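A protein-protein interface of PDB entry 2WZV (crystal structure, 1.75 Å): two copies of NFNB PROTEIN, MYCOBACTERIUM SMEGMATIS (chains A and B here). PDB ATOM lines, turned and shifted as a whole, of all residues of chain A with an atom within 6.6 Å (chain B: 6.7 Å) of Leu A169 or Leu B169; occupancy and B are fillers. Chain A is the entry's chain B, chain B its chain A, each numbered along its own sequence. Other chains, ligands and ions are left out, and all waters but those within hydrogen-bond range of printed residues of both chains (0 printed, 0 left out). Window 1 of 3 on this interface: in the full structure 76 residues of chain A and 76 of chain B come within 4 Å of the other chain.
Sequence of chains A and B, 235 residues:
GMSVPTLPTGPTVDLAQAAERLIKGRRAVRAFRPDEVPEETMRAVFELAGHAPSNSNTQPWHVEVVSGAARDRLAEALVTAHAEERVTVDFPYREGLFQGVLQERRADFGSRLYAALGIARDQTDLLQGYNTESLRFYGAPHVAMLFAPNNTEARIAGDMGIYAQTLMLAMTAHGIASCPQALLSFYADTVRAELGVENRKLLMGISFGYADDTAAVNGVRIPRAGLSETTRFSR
Of the printed residues of chain B, Ile A23 touches Leu B48 (3.5 Å) and Thr B166 (3.6 Å). Ala A164 touches none of the printed residues of chain B. Leu A169 touches just one residue of chain B: Leu B169 (3.8 Å). Printed residues of chain B within 4 Å of Ala A173: Ala B19. Of the printed residues of chain A, Leu B48 touches Ile A23 and Lys A24. Leu B169 touches just one residue of chain A: Leu A169 (3.8 Å). The nearest printed residue of chain B that does not touch Leu A169 is Ile B23 (4.9 Å). The nearest residue of chain A that does not touch Leu B169 is Ala A19 (4.7 Å).
NE2 of Gln B165 lies within hydrogen-bond range of OG1 of Thr A166, at 2.8 Å. OG1 of Thr B166 sits at hydrogen-bond distance from NE2 of Gln A165, at 2.9 Å.
Of the 19 printed residues of chain B, 9 touch a printed residue of chain A. Printed residues of chain B that touch a printed residue of chain A: Ala B19, Leu B22, Ile B23, Lys B24, Leu B48, Gln B165, Thr B166, Leu B169 and Ala B173. Hydrophobic or aromatic side chains of chain B that line the printed part of chain A: Ala B19, Leu B22, Ile B23, Leu B48, Leu B169 and Ala B173. Among the printed residues, 13 pairs touch across the chains. Among the printed residues, no Asp or Glu carboxylate lies within 4 Å of a Lys or Arg side-chain nitrogen of the other chain.
Leu B22 touches Ala A19. Ala A19 touches Ala B173. CD1 of Leu A22 touches CB of Ala B19, at 3.96 Å. Ile A23 touches Leu B48 (CG2 to O, 3.5 Å). CG2 of Ile A23 touches CG2 of Thr B166, 3.6 Å away. Leu B48 touches Lys A24 (CD1 to CG, 3.99 Å). Ile B23 touches Leu A48. Ile B23 touches Thr A166 (CG2 to CG2, 3.6 Å). Leu A169 touches Leu B169 (CD1 to CD1, 3.8 Å). CB of Ala A173 touches CB of Ala B19, 3.5 Å away.
Ala A19 touches Ala B173, and with the chains exchanged Ala A173 touches Ala B19. Ile A23 touches Leu B48, and with the chains exchanged Leu A48 touches Ile B23. Lys A24 touches Leu B48, and with the chains exchanged Leu A48 touches Lys B24. Leu B169 touches its own counterpart, Leu A169. 18 positions are printed for both chains. Of the 13 pairs that touch across the chains among the printed residues, 13 have their exchanged pair printed and touching as well.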
ATOM      1  N   ALA A  19     -17.381 -20.998 -23.782  1.00  0.00           N
ATOM      2  CA  ALA A  19     -16.380 -22.059 -23.615  1.00  0.00           C
ATOM      3  C   ALA A  19     -15.251 -21.871 -24.639  1.00  0.00           C
ATOM      4  O   ALA A  19     -14.096 -22.066 -24.279  1.00  0.00           O
ATOM      5  CB  ALA A  19     -17.013 -23.429 -23.786  1.00  0.00           C
ATOM      6  N   LEU A  22     -13.048 -18.901 -23.359  1.00  0.00           N
ATOM      7  CA  LEU A  22     -12.217 -19.270 -22.221  1.00  0.00           C
ATOM      8  C   LEU A  22     -11.107 -20.229 -22.614  1.00  0.00           C
ATOM      9  O   LEU A  22      -9.952 -20.016 -22.257  1.00  0.00           O
ATOM     10  CB  LEU A  22     -13.075 -19.906 -21.109  1.00  0.00           C
ATOM     11  CG  LEU A  22     -14.138 -18.993 -20.520  1.00  0.00           C
ATOM     12  CD1 LEU A  22     -15.062 -19.764 -19.607  1.00  0.00           C
ATOM     13  CD2 LEU A  22     -13.503 -17.821 -19.799  1.00  0.00           C
ATOM     14  N   ILE A  23     -11.470 -21.308 -23.312  1.00  0.00           N
ATOM     15  CA  ILE A  23     -10.513 -22.364 -23.670  1.00  0.00           C
ATOM     16  C   ILE A  23      -9.450 -21.905 -24.655  1.00  0.00           C
ATOM     17  O   ILE A  23      -8.271 -22.209 -24.444  1.00  0.00           O
ATOM     18  CB  ILE A  23     -11.246 -23.669 -24.079  1.00  0.00           C
ATOM     19  CG1 ILE A  23     -11.949 -24.250 -22.833  1.00  0.00           C
ATOM     20  CG2 ILE A  23     -10.284 -24.714 -24.728  1.00  0.00           C
ATOM     21  CD1 ILE A  23     -13.061 -25.270 -23.147  1.00  0.00           C
ATOM     22  N   LYS A  24      -9.847 -21.162 -25.700  1.00  0.00           N
ATOM     23  CA  LYS A  24      -8.852 -20.640 -26.655  1.00  0.00           C
ATOM     24  C   LYS A  24      -8.198 -19.357 -26.125  1.00  0.00           C
ATOM     25  O   LYS A  24      -7.090 -19.044 -26.536  1.00  0.00           O
ATOM     26  CB  LYS A  24      -9.477 -20.354 -28.029  1.00  0.00           C
ATOM     27  CG  LYS A  24      -9.870 -21.595 -28.802  1.00  0.00           C
ATOM     28  CD  LYS A  24     -10.399 -21.189 -30.181  1.00  0.00           C
ATOM     29  CE  LYS A  24     -10.485 -22.337 -31.139  1.00  0.00           C
ATOM     30  NZ  LYS A  24     -11.264 -21.971 -32.361  1.00  0.00           N
ATOM     31  N   ARG A  26      -7.374 -18.565 -22.937  1.00  0.00           N
ATOM     32  CA  ARG A  26      -6.332 -18.842 -21.953  1.00  0.00           C
ATOM     33  C   ARG A  26      -5.017 -19.166 -22.706  1.00  0.00           C
ATOM     34  O   ARG A  26      -5.000 -20.017 -23.601  1.00  0.00           O
ATOM     35  CB  ARG A  26      -6.721 -20.036 -21.065  1.00  0.00           C
ATOM     36  CG  ARG A  26      -5.635 -20.401 -20.052  1.00  0.00           C
ATOM     37  CD  ARG A  26      -5.451 -21.912 -19.929  1.00  0.00           C
ATOM     38  NE  ARG A  26      -5.082 -22.534 -21.213  1.00  0.00           N
ATOM     39  CZ  ARG A  26      -3.866 -22.512 -21.754  1.00  0.00           C
ATOM     40  NH1 ARG A  26      -2.851 -21.919 -21.117  1.00  0.00           N
ATOM     41  NH2 ARG A  26      -3.654 -23.068 -22.941  1.00  0.00           N
ATOM     42  N   LEU A  48     -14.523 -21.116  -7.147  1.00  0.00           N
ATOM     43  CA  LEU A  48     -15.026 -21.750  -8.370  1.00  0.00           C
ATOM     44  C   LEU A  48     -14.169 -22.945  -8.753  1.00  0.00           C
ATOM     45  O   LEU A  48     -14.705 -24.007  -9.115  1.00  0.00           O
ATOM     46  CB  LEU A  48     -15.116 -20.743  -9.536  1.00  0.00           C
ATOM     47  CG  LEU A  48     -15.771 -21.282 -10.830  1.00  0.00           C
ATOM     48  CD1 LEU A  48     -17.129 -21.988 -10.540  1.00  0.00           C
ATOM     49  CD2 LEU A  48     -15.932 -20.179 -11.856  1.00  0.00           C
ATOM     50  N   ALA A 164      -6.083 -27.803 -12.032  1.00  0.00           N
ATOM     51  CA  ALA A 164      -5.250 -26.722 -12.599  1.00  0.00           C
ATOM     52  C   ALA A 164      -5.959 -26.050 -13.774  1.00  0.00           C
ATOM     53  O   ALA A 164      -6.013 -24.827 -13.823  1.00  0.00           O
ATOM     54  CB  ALA A 164      -3.885 -27.259 -13.028  1.00  0.00           C
ATOM     55  N   GLN A 165      -6.562 -26.843 -14.665  1.00  0.00           N
ATOM     56  CA  GLN A 165      -7.272 -26.296 -15.822  1.00  0.00           C
ATOM     57  C   GLN A 165      -8.556 -25.567 -15.386  1.00  0.00           C
ATOM     58  O   GLN A 165      -8.864 -24.508 -15.944  1.00  0.00           O
ATOM     59  CB  GLN A 165      -7.546 -27.378 -16.903  1.00  0.00           C
ATOM     60  CG  GLN A 165      -8.279 -26.838 -18.153  1.00  0.00           C
ATOM     61  CD  GLN A 165      -7.484 -25.879 -19.033  1.00  0.00           C
ATOM     62  OE1 GLN A 165      -6.557 -25.166 -18.595  1.00  0.00           O
ATOM     63  NE2 GLN A 165      -7.865 -25.818 -20.315  1.00  0.00           N
ATOM     64  N   THR A 166      -9.281 -26.098 -14.384  1.00  0.00           N
ATOM     65  CA  THR A 166     -10.485 -25.410 -13.888  1.00  0.00           C
ATOM     66  C   THR A 166     -10.090 -24.025 -13.356  1.00  0.00           C
ATOM     67  O   THR A 166     -10.729 -23.011 -13.678  1.00  0.00           O
ATOM     68  CB  THR A 166     -11.173 -26.246 -12.775  1.00  0.00           C
ATOM     69  OG1 THR A 166     -11.414 -27.582 -13.247  1.00  0.00           O
ATOM     70  CG2 THR A 166     -12.499 -25.627 -12.336  1.00  0.00           C
ATOM     71  N   LEU A 167      -9.014 -23.985 -12.574  1.00  0.00           N
ATOM     72  CA  LEU A 167      -8.485 -22.740 -12.024  1.00  0.00           C
ATOM     73  C   LEU A 167      -8.064 -21.755 -13.119  1.00  0.00           C
ATOM     74  O   LEU A 167      -8.447 -20.593 -13.059  1.00  0.00           O
ATOM     75  CB  LEU A 167      -7.299 -23.063 -11.100  1.00  0.00           C
ATOM     76  CG  LEU A 167      -6.671 -21.827 -10.426  1.00  0.00           C
ATOM     77  CD1 LEU A 167      -7.719 -21.079  -9.560  1.00  0.00           C
ATOM     78  CD2 LEU A 167      -5.410 -22.207  -9.638  1.00  0.00           C
ATOM     79  N   MET A 168      -7.294 -22.215 -14.115  1.00  0.00           N
ATOM     80  CA  MET A 168      -6.810 -21.329 -15.188  1.00  0.00           C
ATOM     81  C   MET A 168      -7.964 -20.761 -16.007  1.00  0.00           C
ATOM     82  O   MET A 168      -7.940 -19.587 -16.367  1.00  0.00           O
ATOM     83  CB  MET A 168      -5.776 -22.083 -16.056  1.00  0.00           C
ATOM     84  CG  MET A 168      -4.468 -22.269 -15.282  1.00  0.00           C
ATOM     85  SD  MET A 168      -3.070 -22.905 -16.440  1.00  0.00           S
ATOM     86  CE  MET A 168      -3.604 -24.823 -16.517  1.00  0.00           C
ATOM     87  N   LEU A 169      -9.007 -21.572 -16.252  1.00  0.00           N
ATOM     88  CA  LEU A 169     -10.172 -21.103 -17.003  1.00  0.00           C
ATOM     89  C   LEU A 169     -10.992 -20.127 -16.150  1.00  0.00           C
ATOM     90  O   LEU A 169     -11.453 -19.115 -16.676  1.00  0.00           O
ATOM     91  CB  LEU A 169     -11.012 -22.285 -17.481  1.00  0.00           C
ATOM     92  CG  LEU A 169     -10.313 -23.210 -18.501  1.00  0.00           C
ATOM     93  CD1 LEU A 169     -11.228 -24.394 -18.862  1.00  0.00           C
ATOM     94  CD2 LEU A 169      -9.940 -22.440 -19.812  1.00  0.00           C
ATOM     95  N   ALA A 170     -11.133 -20.388 -14.837  1.00  0.00           N
ATOM     96  CA  ALA A 170     -11.858 -19.435 -13.959  1.00  0.00           C
ATOM     97  C   ALA A 170     -11.082 -18.088 -13.925  1.00  0.00           C
ATOM     98  O   ALA A 170     -11.697 -17.008 -13.957  1.00  0.00           O
ATOM     99  CB  ALA A 170     -11.990 -20.005 -12.549  1.00  0.00           C
ATOM    100  N   MET A 171      -9.745 -18.156 -13.921  1.00  0.00           N
ATOM    101  CA  MET A 171      -8.900 -16.949 -13.958  1.00  0.00           C
ATOM    102  C   MET A 171      -9.128 -16.192 -15.266  1.00  0.00           C
ATOM    103  O   MET A 171      -9.427 -14.998 -15.248  1.00  0.00           O
ATOM    104  CB  MET A 171      -7.415 -17.305 -13.835  1.00  0.00           C
ATOM    105  CG  MET A 171      -7.008 -17.707 -12.410  1.00  0.00           C
ATOM    106  SD  MET A 171      -5.188 -18.362 -12.489  1.00  0.00           S
ATOM    107  CE  MET A 171      -4.948 -18.550 -10.505  1.00  0.00           C
ATOM    108  N   THR A 172      -9.114 -16.916 -16.387  1.00  0.00           N
ATOM    109  CA  THR A 172      -9.300 -16.313 -17.718  1.00  0.00           C
ATOM    110  C   THR A 172     -10.643 -15.563 -17.809  1.00  0.00           C
ATOM    111  O   THR A 172     -10.716 -14.481 -18.410  1.00  0.00           O
ATOM    112  CB  THR A 172      -9.154 -17.398 -18.799  1.00  0.00           C
ATOM    113  OG1 THR A 172      -7.838 -17.959 -18.732  1.00  0.00           O
ATOM    114  CG2 THR A 172      -9.404 -16.864 -20.232  1.00  0.00           C
ATOM    115  N   ALA A 173     -11.695 -16.138 -17.186  1.00  0.00           N
ATOM    116  CA  ALA A 173     -13.042 -15.547 -17.152  1.00  0.00           C
ATOM    117  C   ALA A 173     -13.064 -14.173 -16.482  1.00  0.00           C
ATOM    118  O   ALA A 173     -13.935 -13.355 -16.803  1.00  0.00           O
ATOM    119  CB  ALA A 173     -13.998 -16.479 -16.450  1.00  0.00           C
ATOM    120  N   HIS A 174     -12.130 -13.938 -15.548  1.00  0.00           N
ATOM    121  CA  HIS A 174     -11.992 -12.675 -14.830  1.00  0.00           C
ATOM    122  C   HIS A 174     -10.863 -11.777 -15.385  1.00  0.00           C
ATOM    123  O   HIS A 174     -10.476 -10.801 -14.725  1.00  0.00           O
ATOM    124  CB  HIS A 174     -11.826 -12.931 -13.311  1.00  0.00           C
ATOM    125  CG  HIS A 174     -13.049 -13.514 -12.687  1.00  0.00           C
ATOM    126  ND1 HIS A 174     -14.009 -12.704 -12.067  1.00  0.00           N
ATOM    127  CD2 HIS A 174     -13.478 -14.798 -12.665  1.00  0.00           C
ATOM    128  CE1 HIS A 174     -14.958 -13.531 -11.652  1.00  0.00           C
ATOM    129  NE2 HIS A 174     -14.694 -14.800 -12.007  1.00  0.00           N
ATOM    130  N   SER A 178      -2.406 -16.247 -16.659  1.00  0.00           N
ATOM    131  CA  SER A 178      -1.677 -17.219 -15.826  1.00  0.00           C
ATOM    132  C   SER A 178      -0.571 -17.895 -16.643  1.00  0.00           C
ATOM    133  O   SER A 178      -0.578 -17.866 -17.878  1.00  0.00           O
ATOM    134  CB  SER A 178      -2.640 -18.294 -15.306  1.00  0.00           C
ATOM    135  OG  SER A 178      -3.287 -18.943 -16.402  1.00  0.00           O
ATOM    136  N   ALA B  19     -18.523 -18.863 -16.965  1.00  0.00           N
ATOM    137  CA  ALA B  19     -17.564 -19.776 -16.341  1.00  0.00           C
ATOM    138  C   ALA B  19     -18.201 -20.474 -15.138  1.00  0.00           C
ATOM    139  O   ALA B  19     -18.020 -21.677 -14.984  1.00  0.00           O
ATOM    140  CB  ALA B  19     -16.301 -19.033 -15.917  1.00  0.00           C
ATOM    141  N   LEU B  22     -20.653 -23.128 -16.434  1.00  0.00           N
ATOM    142  CA  LEU B  22     -19.963 -24.291 -16.998  1.00  0.00           C
ATOM    143  C   LEU B  22     -19.367 -25.155 -15.923  1.00  0.00           C
ATOM    144  O   LEU B  22     -19.576 -26.365 -15.907  1.00  0.00           O
ATOM    145  CB  LEU B  22     -18.828 -23.876 -17.971  1.00  0.00           C
ATOM    146  CG  LEU B  22     -19.243 -23.215 -19.263  1.00  0.00           C
ATOM    147  CD1 LEU B  22     -18.028 -22.696 -20.005  1.00  0.00           C
ATOM    148  CD2 LEU B  22     -20.064 -24.165 -20.116  1.00  0.00           C
ATOM    149  N   ILE B  23     -18.586 -24.536 -15.047  1.00  0.00           N
ATOM    150  CA  ILE B  23     -17.825 -25.250 -14.025  1.00  0.00           C
ATOM    151  C   ILE B  23     -18.729 -25.866 -12.963  1.00  0.00           C
ATOM    152  O   ILE B  23     -18.503 -26.998 -12.538  1.00  0.00           O
ATOM    153  CB  ILE B  23     -16.676 -24.370 -13.466  1.00  0.00           C
ATOM    154  CG1 ILE B  23     -15.614 -24.098 -14.584  1.00  0.00           C
ATOM    155  CG2 ILE B  23     -16.045 -25.034 -12.222  1.00  0.00           C
ATOM    156  CD1 ILE B  23     -14.673 -22.898 -14.280  1.00  0.00           C
ATOM    157  N   LYS B  24     -19.749 -25.116 -12.535  1.00  0.00           N
ATOM    158  CA  LYS B  24     -20.678 -25.650 -11.554  1.00  0.00           C
ATOM    159  C   LYS B  24     -21.751 -26.536 -12.188  1.00  0.00           C
ATOM    160  O   LYS B  24     -22.223 -27.461 -11.533  1.00  0.00           O
ATOM    161  CB  LYS B  24     -21.312 -24.532 -10.723  1.00  0.00           C
ATOM    162  CG  LYS B  24     -20.313 -23.931  -9.738  1.00  0.00           C
ATOM    163  CD  LYS B  24     -20.945 -22.786  -8.911  1.00  0.00           C
ATOM    164  CE  LYS B  24     -21.856 -23.251  -7.800  1.00  0.00           C
ATOM    165  NZ  LYS B  24     -22.523 -22.104  -7.121  1.00  0.00           N
ATOM    166  N   ARG B  26     -21.424 -28.616 -14.841  1.00  0.00           N
ATOM    167  CA  ARG B  26     -20.894 -29.943 -15.165  1.00  0.00           C
ATOM    168  C   ARG B  26     -20.999 -30.832 -13.914  1.00  0.00           C
ATOM    169  O   ARG B  26     -20.542 -30.442 -12.840  1.00  0.00           O
ATOM    170  CB  ARG B  26     -19.414 -29.847 -15.612  1.00  0.00           C
ATOM    171  CG  ARG B  26     -18.770 -31.217 -15.977  1.00  0.00           C
ATOM    172  CD  ARG B  26     -17.380 -31.457 -15.369  1.00  0.00           C
ATOM    173  NE  ARG B  26     -17.361 -31.233 -13.912  1.00  0.00           N
ATOM    174  CZ  ARG B  26     -17.754 -32.108 -12.993  1.00  0.00           C
ATOM    175  NH1 ARG B  26     -18.156 -33.329 -13.352  1.00  0.00           N
ATOM    176  NH2 ARG B  26     -17.754 -31.772 -11.704  1.00  0.00           N
ATOM    177  N   LEU B  48     -12.068 -28.341 -29.806  1.00  0.00           N
ATOM    178  CA  LEU B  48     -11.904 -27.359 -28.735  1.00  0.00           C
ATOM    179  C   LEU B  48     -11.077 -27.929 -27.576  1.00  0.00           C
ATOM    180  O   LEU B  48     -10.165 -27.251 -27.101  1.00  0.00           O
ATOM    181  CB  LEU B  48     -13.266 -26.849 -28.235  1.00  0.00           C
ATOM    182  CG  LEU B  48     -13.183 -25.712 -27.209  1.00  0.00           C
ATOM    183  CD1 LEU B  48     -12.350 -24.544 -27.751  1.00  0.00           C
ATOM    184  CD2 LEU B  48     -14.580 -25.267 -26.775  1.00  0.00           C
ATOM    185  N   ALA B 164      -8.879 -33.795 -19.959  1.00  0.00           N
ATOM    186  CA  ALA B 164     -10.176 -34.380 -19.561  1.00  0.00           C
ATOM    187  C   ALA B 164     -11.141 -33.274 -19.098  1.00  0.00           C
ATOM    188  O   ALA B 164     -12.281 -33.270 -19.518  1.00  0.00           O
ATOM    189  CB  ALA B 164      -9.970 -35.381 -18.430  1.00  0.00           C
ATOM    190  N   GLN B 165     -10.675 -32.332 -18.282  1.00  0.00           N
ATOM    191  CA  GLN B 165     -11.550 -31.257 -17.792  1.00  0.00           C
ATOM    192  C   GLN B 165     -11.881 -30.285 -18.921  1.00  0.00           C
ATOM    193  O   GLN B 165     -13.016 -29.803 -18.989  1.00  0.00           O
ATOM    194  CB  GLN B 165     -10.924 -30.527 -16.588  1.00  0.00           C
ATOM    195  CG  GLN B 165     -11.778 -29.378 -15.999  1.00  0.00           C
ATOM    196  CD  GLN B 165     -13.084 -29.797 -15.315  1.00  0.00           C
ATOM    197  OE1 GLN B 165     -13.671 -30.851 -15.620  1.00  0.00           O
ATOM    198  NE2 GLN B 165     -13.628 -28.916 -14.438  1.00  0.00           N
ATOM    199  N   THR B 166     -10.922 -29.996 -19.807  1.00  0.00           N
ATOM    200  CA  THR B 166     -11.216 -29.131 -20.963  1.00  0.00           C
ATOM    201  C   THR B 166     -12.340 -29.766 -21.779  1.00  0.00           C
ATOM    202  O   THR B 166     -13.262 -29.073 -22.204  1.00  0.00           O
ATOM    203  CB  THR B 166      -9.985 -28.913 -21.857  1.00  0.00           C
ATOM    204  OG1 THR B 166      -8.906 -28.459 -21.036  1.00  0.00           O
ATOM    205  CG2 THR B 166     -10.235 -27.804 -22.896  1.00  0.00           C
ATOM    206  N   LEU B 167     -12.233 -31.079 -22.019  1.00  0.00           N
ATOM    207  CA  LEU B 167     -13.229 -31.797 -22.795  1.00  0.00           C
ATOM    208  C   LEU B 167     -14.594 -31.773 -22.104  1.00  0.00           C
ATOM    209  O   LEU B 167     -15.588 -31.493 -22.760  1.00  0.00           O
ATOM    210  CB  LEU B 167     -12.770 -33.243 -22.997  1.00  0.00           C
ATOM    211  CG  LEU B 167     -13.724 -34.120 -23.798  1.00  0.00           C
ATOM    212  CD1 LEU B 167     -13.905 -33.546 -25.239  1.00  0.00           C
ATOM    213  CD2 LEU B 167     -13.219 -35.566 -23.823  1.00  0.00           C
ATOM    214  N   MET B 168     -14.644 -32.083 -20.793  1.00  0.00           N
ATOM    215  CA  MET B 168     -15.926 -32.128 -20.082  1.00  0.00           C
ATOM    216  C   MET B 168     -16.621 -30.759 -20.062  1.00  0.00           C
ATOM    217  O   MET B 168     -17.849 -30.681 -20.150  1.00  0.00           O
ATOM    218  CB  MET B 168     -15.747 -32.705 -18.677  1.00  0.00           C
ATOM    219  CG  MET B 168     -15.452 -34.205 -18.723  1.00  0.00           C
ATOM    220  SD  MET B 168     -15.412 -34.949 -16.929  1.00  0.00           S
ATOM    221  CE  MET B 168     -13.625 -34.295 -16.329  1.00  0.00           C
ATOM    222  N   LEU B 169     -15.829 -29.680 -19.938  1.00  0.00           N
ATOM    223  CA  LEU B 169     -16.393 -28.332 -19.943  1.00  0.00           C
ATOM    224  C   LEU B 169     -16.878 -27.951 -21.362  1.00  0.00           C
ATOM    225  O   LEU B 169     -17.960 -27.377 -21.496  1.00  0.00           O
ATOM    226  CB  LEU B 169     -15.376 -27.337 -19.383  1.00  0.00           C
ATOM    227  CG  LEU B 169     -15.069 -27.525 -17.869  1.00  0.00           C
ATOM    228  CD1 LEU B 169     -13.979 -26.550 -17.400  1.00  0.00           C
ATOM    229  CD2 LEU B 169     -16.349 -27.333 -16.993  1.00  0.00           C
ATOM    230  N   ALA B 170     -16.118 -28.330 -22.413  1.00  0.00           N
ATOM    231  CA  ALA B 170     -16.535 -28.091 -23.812  1.00  0.00           C
ATOM    232  C   ALA B 170     -17.870 -28.843 -24.052  1.00  0.00           C
ATOM    233  O   ALA B 170     -18.783 -28.283 -24.657  1.00  0.00           O
ATOM    234  CB  ALA B 170     -15.455 -28.571 -24.789  1.00  0.00           C
ATOM    235  N   MET B 171     -18.009 -30.065 -23.484  1.00  0.00           N
ATOM    236  CA  MET B 171     -19.244 -30.855 -23.602  1.00  0.00           C
ATOM    237  C   MET B 171     -20.393 -30.128 -22.889  1.00  0.00           C
ATOM    238  O   MET B 171     -21.438 -29.880 -23.506  1.00  0.00           O
ATOM    239  CB  MET B 171     -19.072 -32.263 -23.009  1.00  0.00           C
ATOM    240  CG  MET B 171     -18.162 -33.169 -23.843  1.00  0.00           C
ATOM    241  SD  MET B 171     -17.827 -34.794 -22.883  1.00  0.00           S
ATOM    242  CE  MET B 171     -16.926 -35.743 -24.452  1.00  0.00           C
ATOM    243  N   THR B 172     -20.173 -29.719 -21.627  1.00  0.00           N
ATOM    244  CA  THR B 172     -21.182 -28.998 -20.864  1.00  0.00           C
ATOM    245  C   THR B 172     -21.690 -27.759 -21.632  1.00  0.00           C
ATOM    246  O   THR B 172     -22.893 -27.504 -21.641  1.00  0.00           O
ATOM    247  CB  THR B 172     -20.660 -28.643 -19.462  1.00  0.00           C
ATOM    248  OG1 THR B 172     -20.336 -29.862 -18.797  1.00  0.00           O
ATOM    249  CG2 THR B 172     -21.713 -27.890 -18.630  1.00  0.00           C
ATOM    250  N   ALA B 173     -20.772 -27.024 -22.316  1.00  0.00           N
ATOM    251  CA  ALA B 173     -21.130 -25.811 -23.073  1.00  0.00           C
ATOM    252  C   ALA B 173     -22.132 -26.089 -24.199  1.00  0.00           C
ATOM    253  O   ALA B 173     -22.830 -25.171 -24.616  1.00  0.00           O
ATOM    254  CB  ALA B 173     -19.880 -25.180 -23.662  1.00  0.00           C
ATOM    255  N   HIS B 174     -22.149 -27.331 -24.723  1.00  0.00           N
ATOM    256  CA  HIS B 174     -23.060 -27.735 -25.804  1.00  0.00           C
ATOM    257  C   HIS B 174     -24.234 -28.564 -25.270  1.00  0.00           C
ATOM    258  O   HIS B 174     -24.906 -29.243 -26.049  1.00  0.00           O
ATOM    259  CB  HIS B 174     -22.266 -28.504 -26.895  1.00  0.00           C
ATOM    260  CG  HIS B 174     -21.345 -27.616 -27.678  1.00  0.00           C
ATOM    261  ND1 HIS B 174     -21.754 -27.021 -28.856  1.00  0.00           N
ATOM    262  CD2 HIS B 174     -20.106 -27.165 -27.368  1.00  0.00           C
ATOM    263  CE1 HIS B 174     -20.733 -26.277 -29.259  1.00  0.00           C
ATOM    264  NE2 HIS B 174     -19.729 -26.307 -28.384  1.00  0.00           N
ATOM    265  N   ILE B 176     -24.034 -31.175 -23.390  1.00  0.00           N
ATOM    266  CA  ILE B 176     -23.676 -32.591 -23.401  1.00  0.00           C
ATOM    267  C   ILE B 176     -23.244 -33.005 -21.982  1.00  0.00           C
ATOM    268  O   ILE B 176     -22.298 -32.439 -21.426  1.00  0.00           O
ATOM    269  CB  ILE B 176     -22.567 -32.874 -24.448  1.00  0.00           C
ATOM    270  CG1 ILE B 176     -23.055 -32.537 -25.900  1.00  0.00           C
ATOM    271  CG2 ILE B 176     -22.081 -34.326 -24.330  1.00  0.00           C
ATOM    272  CD1 ILE B 176     -21.856 -32.362 -26.931  1.00  0.00           C
ATOM    273  N   SER B 178     -21.781 -35.754 -19.144  1.00  0.00           N
ATOM    274  CA  SER B 178     -20.669 -36.697 -19.159  1.00  0.00           C
ATOM    275  C   SER B 178     -20.455 -37.317 -17.801  1.00  0.00           C
ATOM    276  O   SER B 178     -20.928 -36.785 -16.797  1.00  0.00           O
ATOM    277  CB  SER B 178     -19.385 -36.000 -19.618  1.00  0.00           C
ATOM    278  OG  SER B 178     -18.985 -34.982 -18.708  1.00  0.00           O
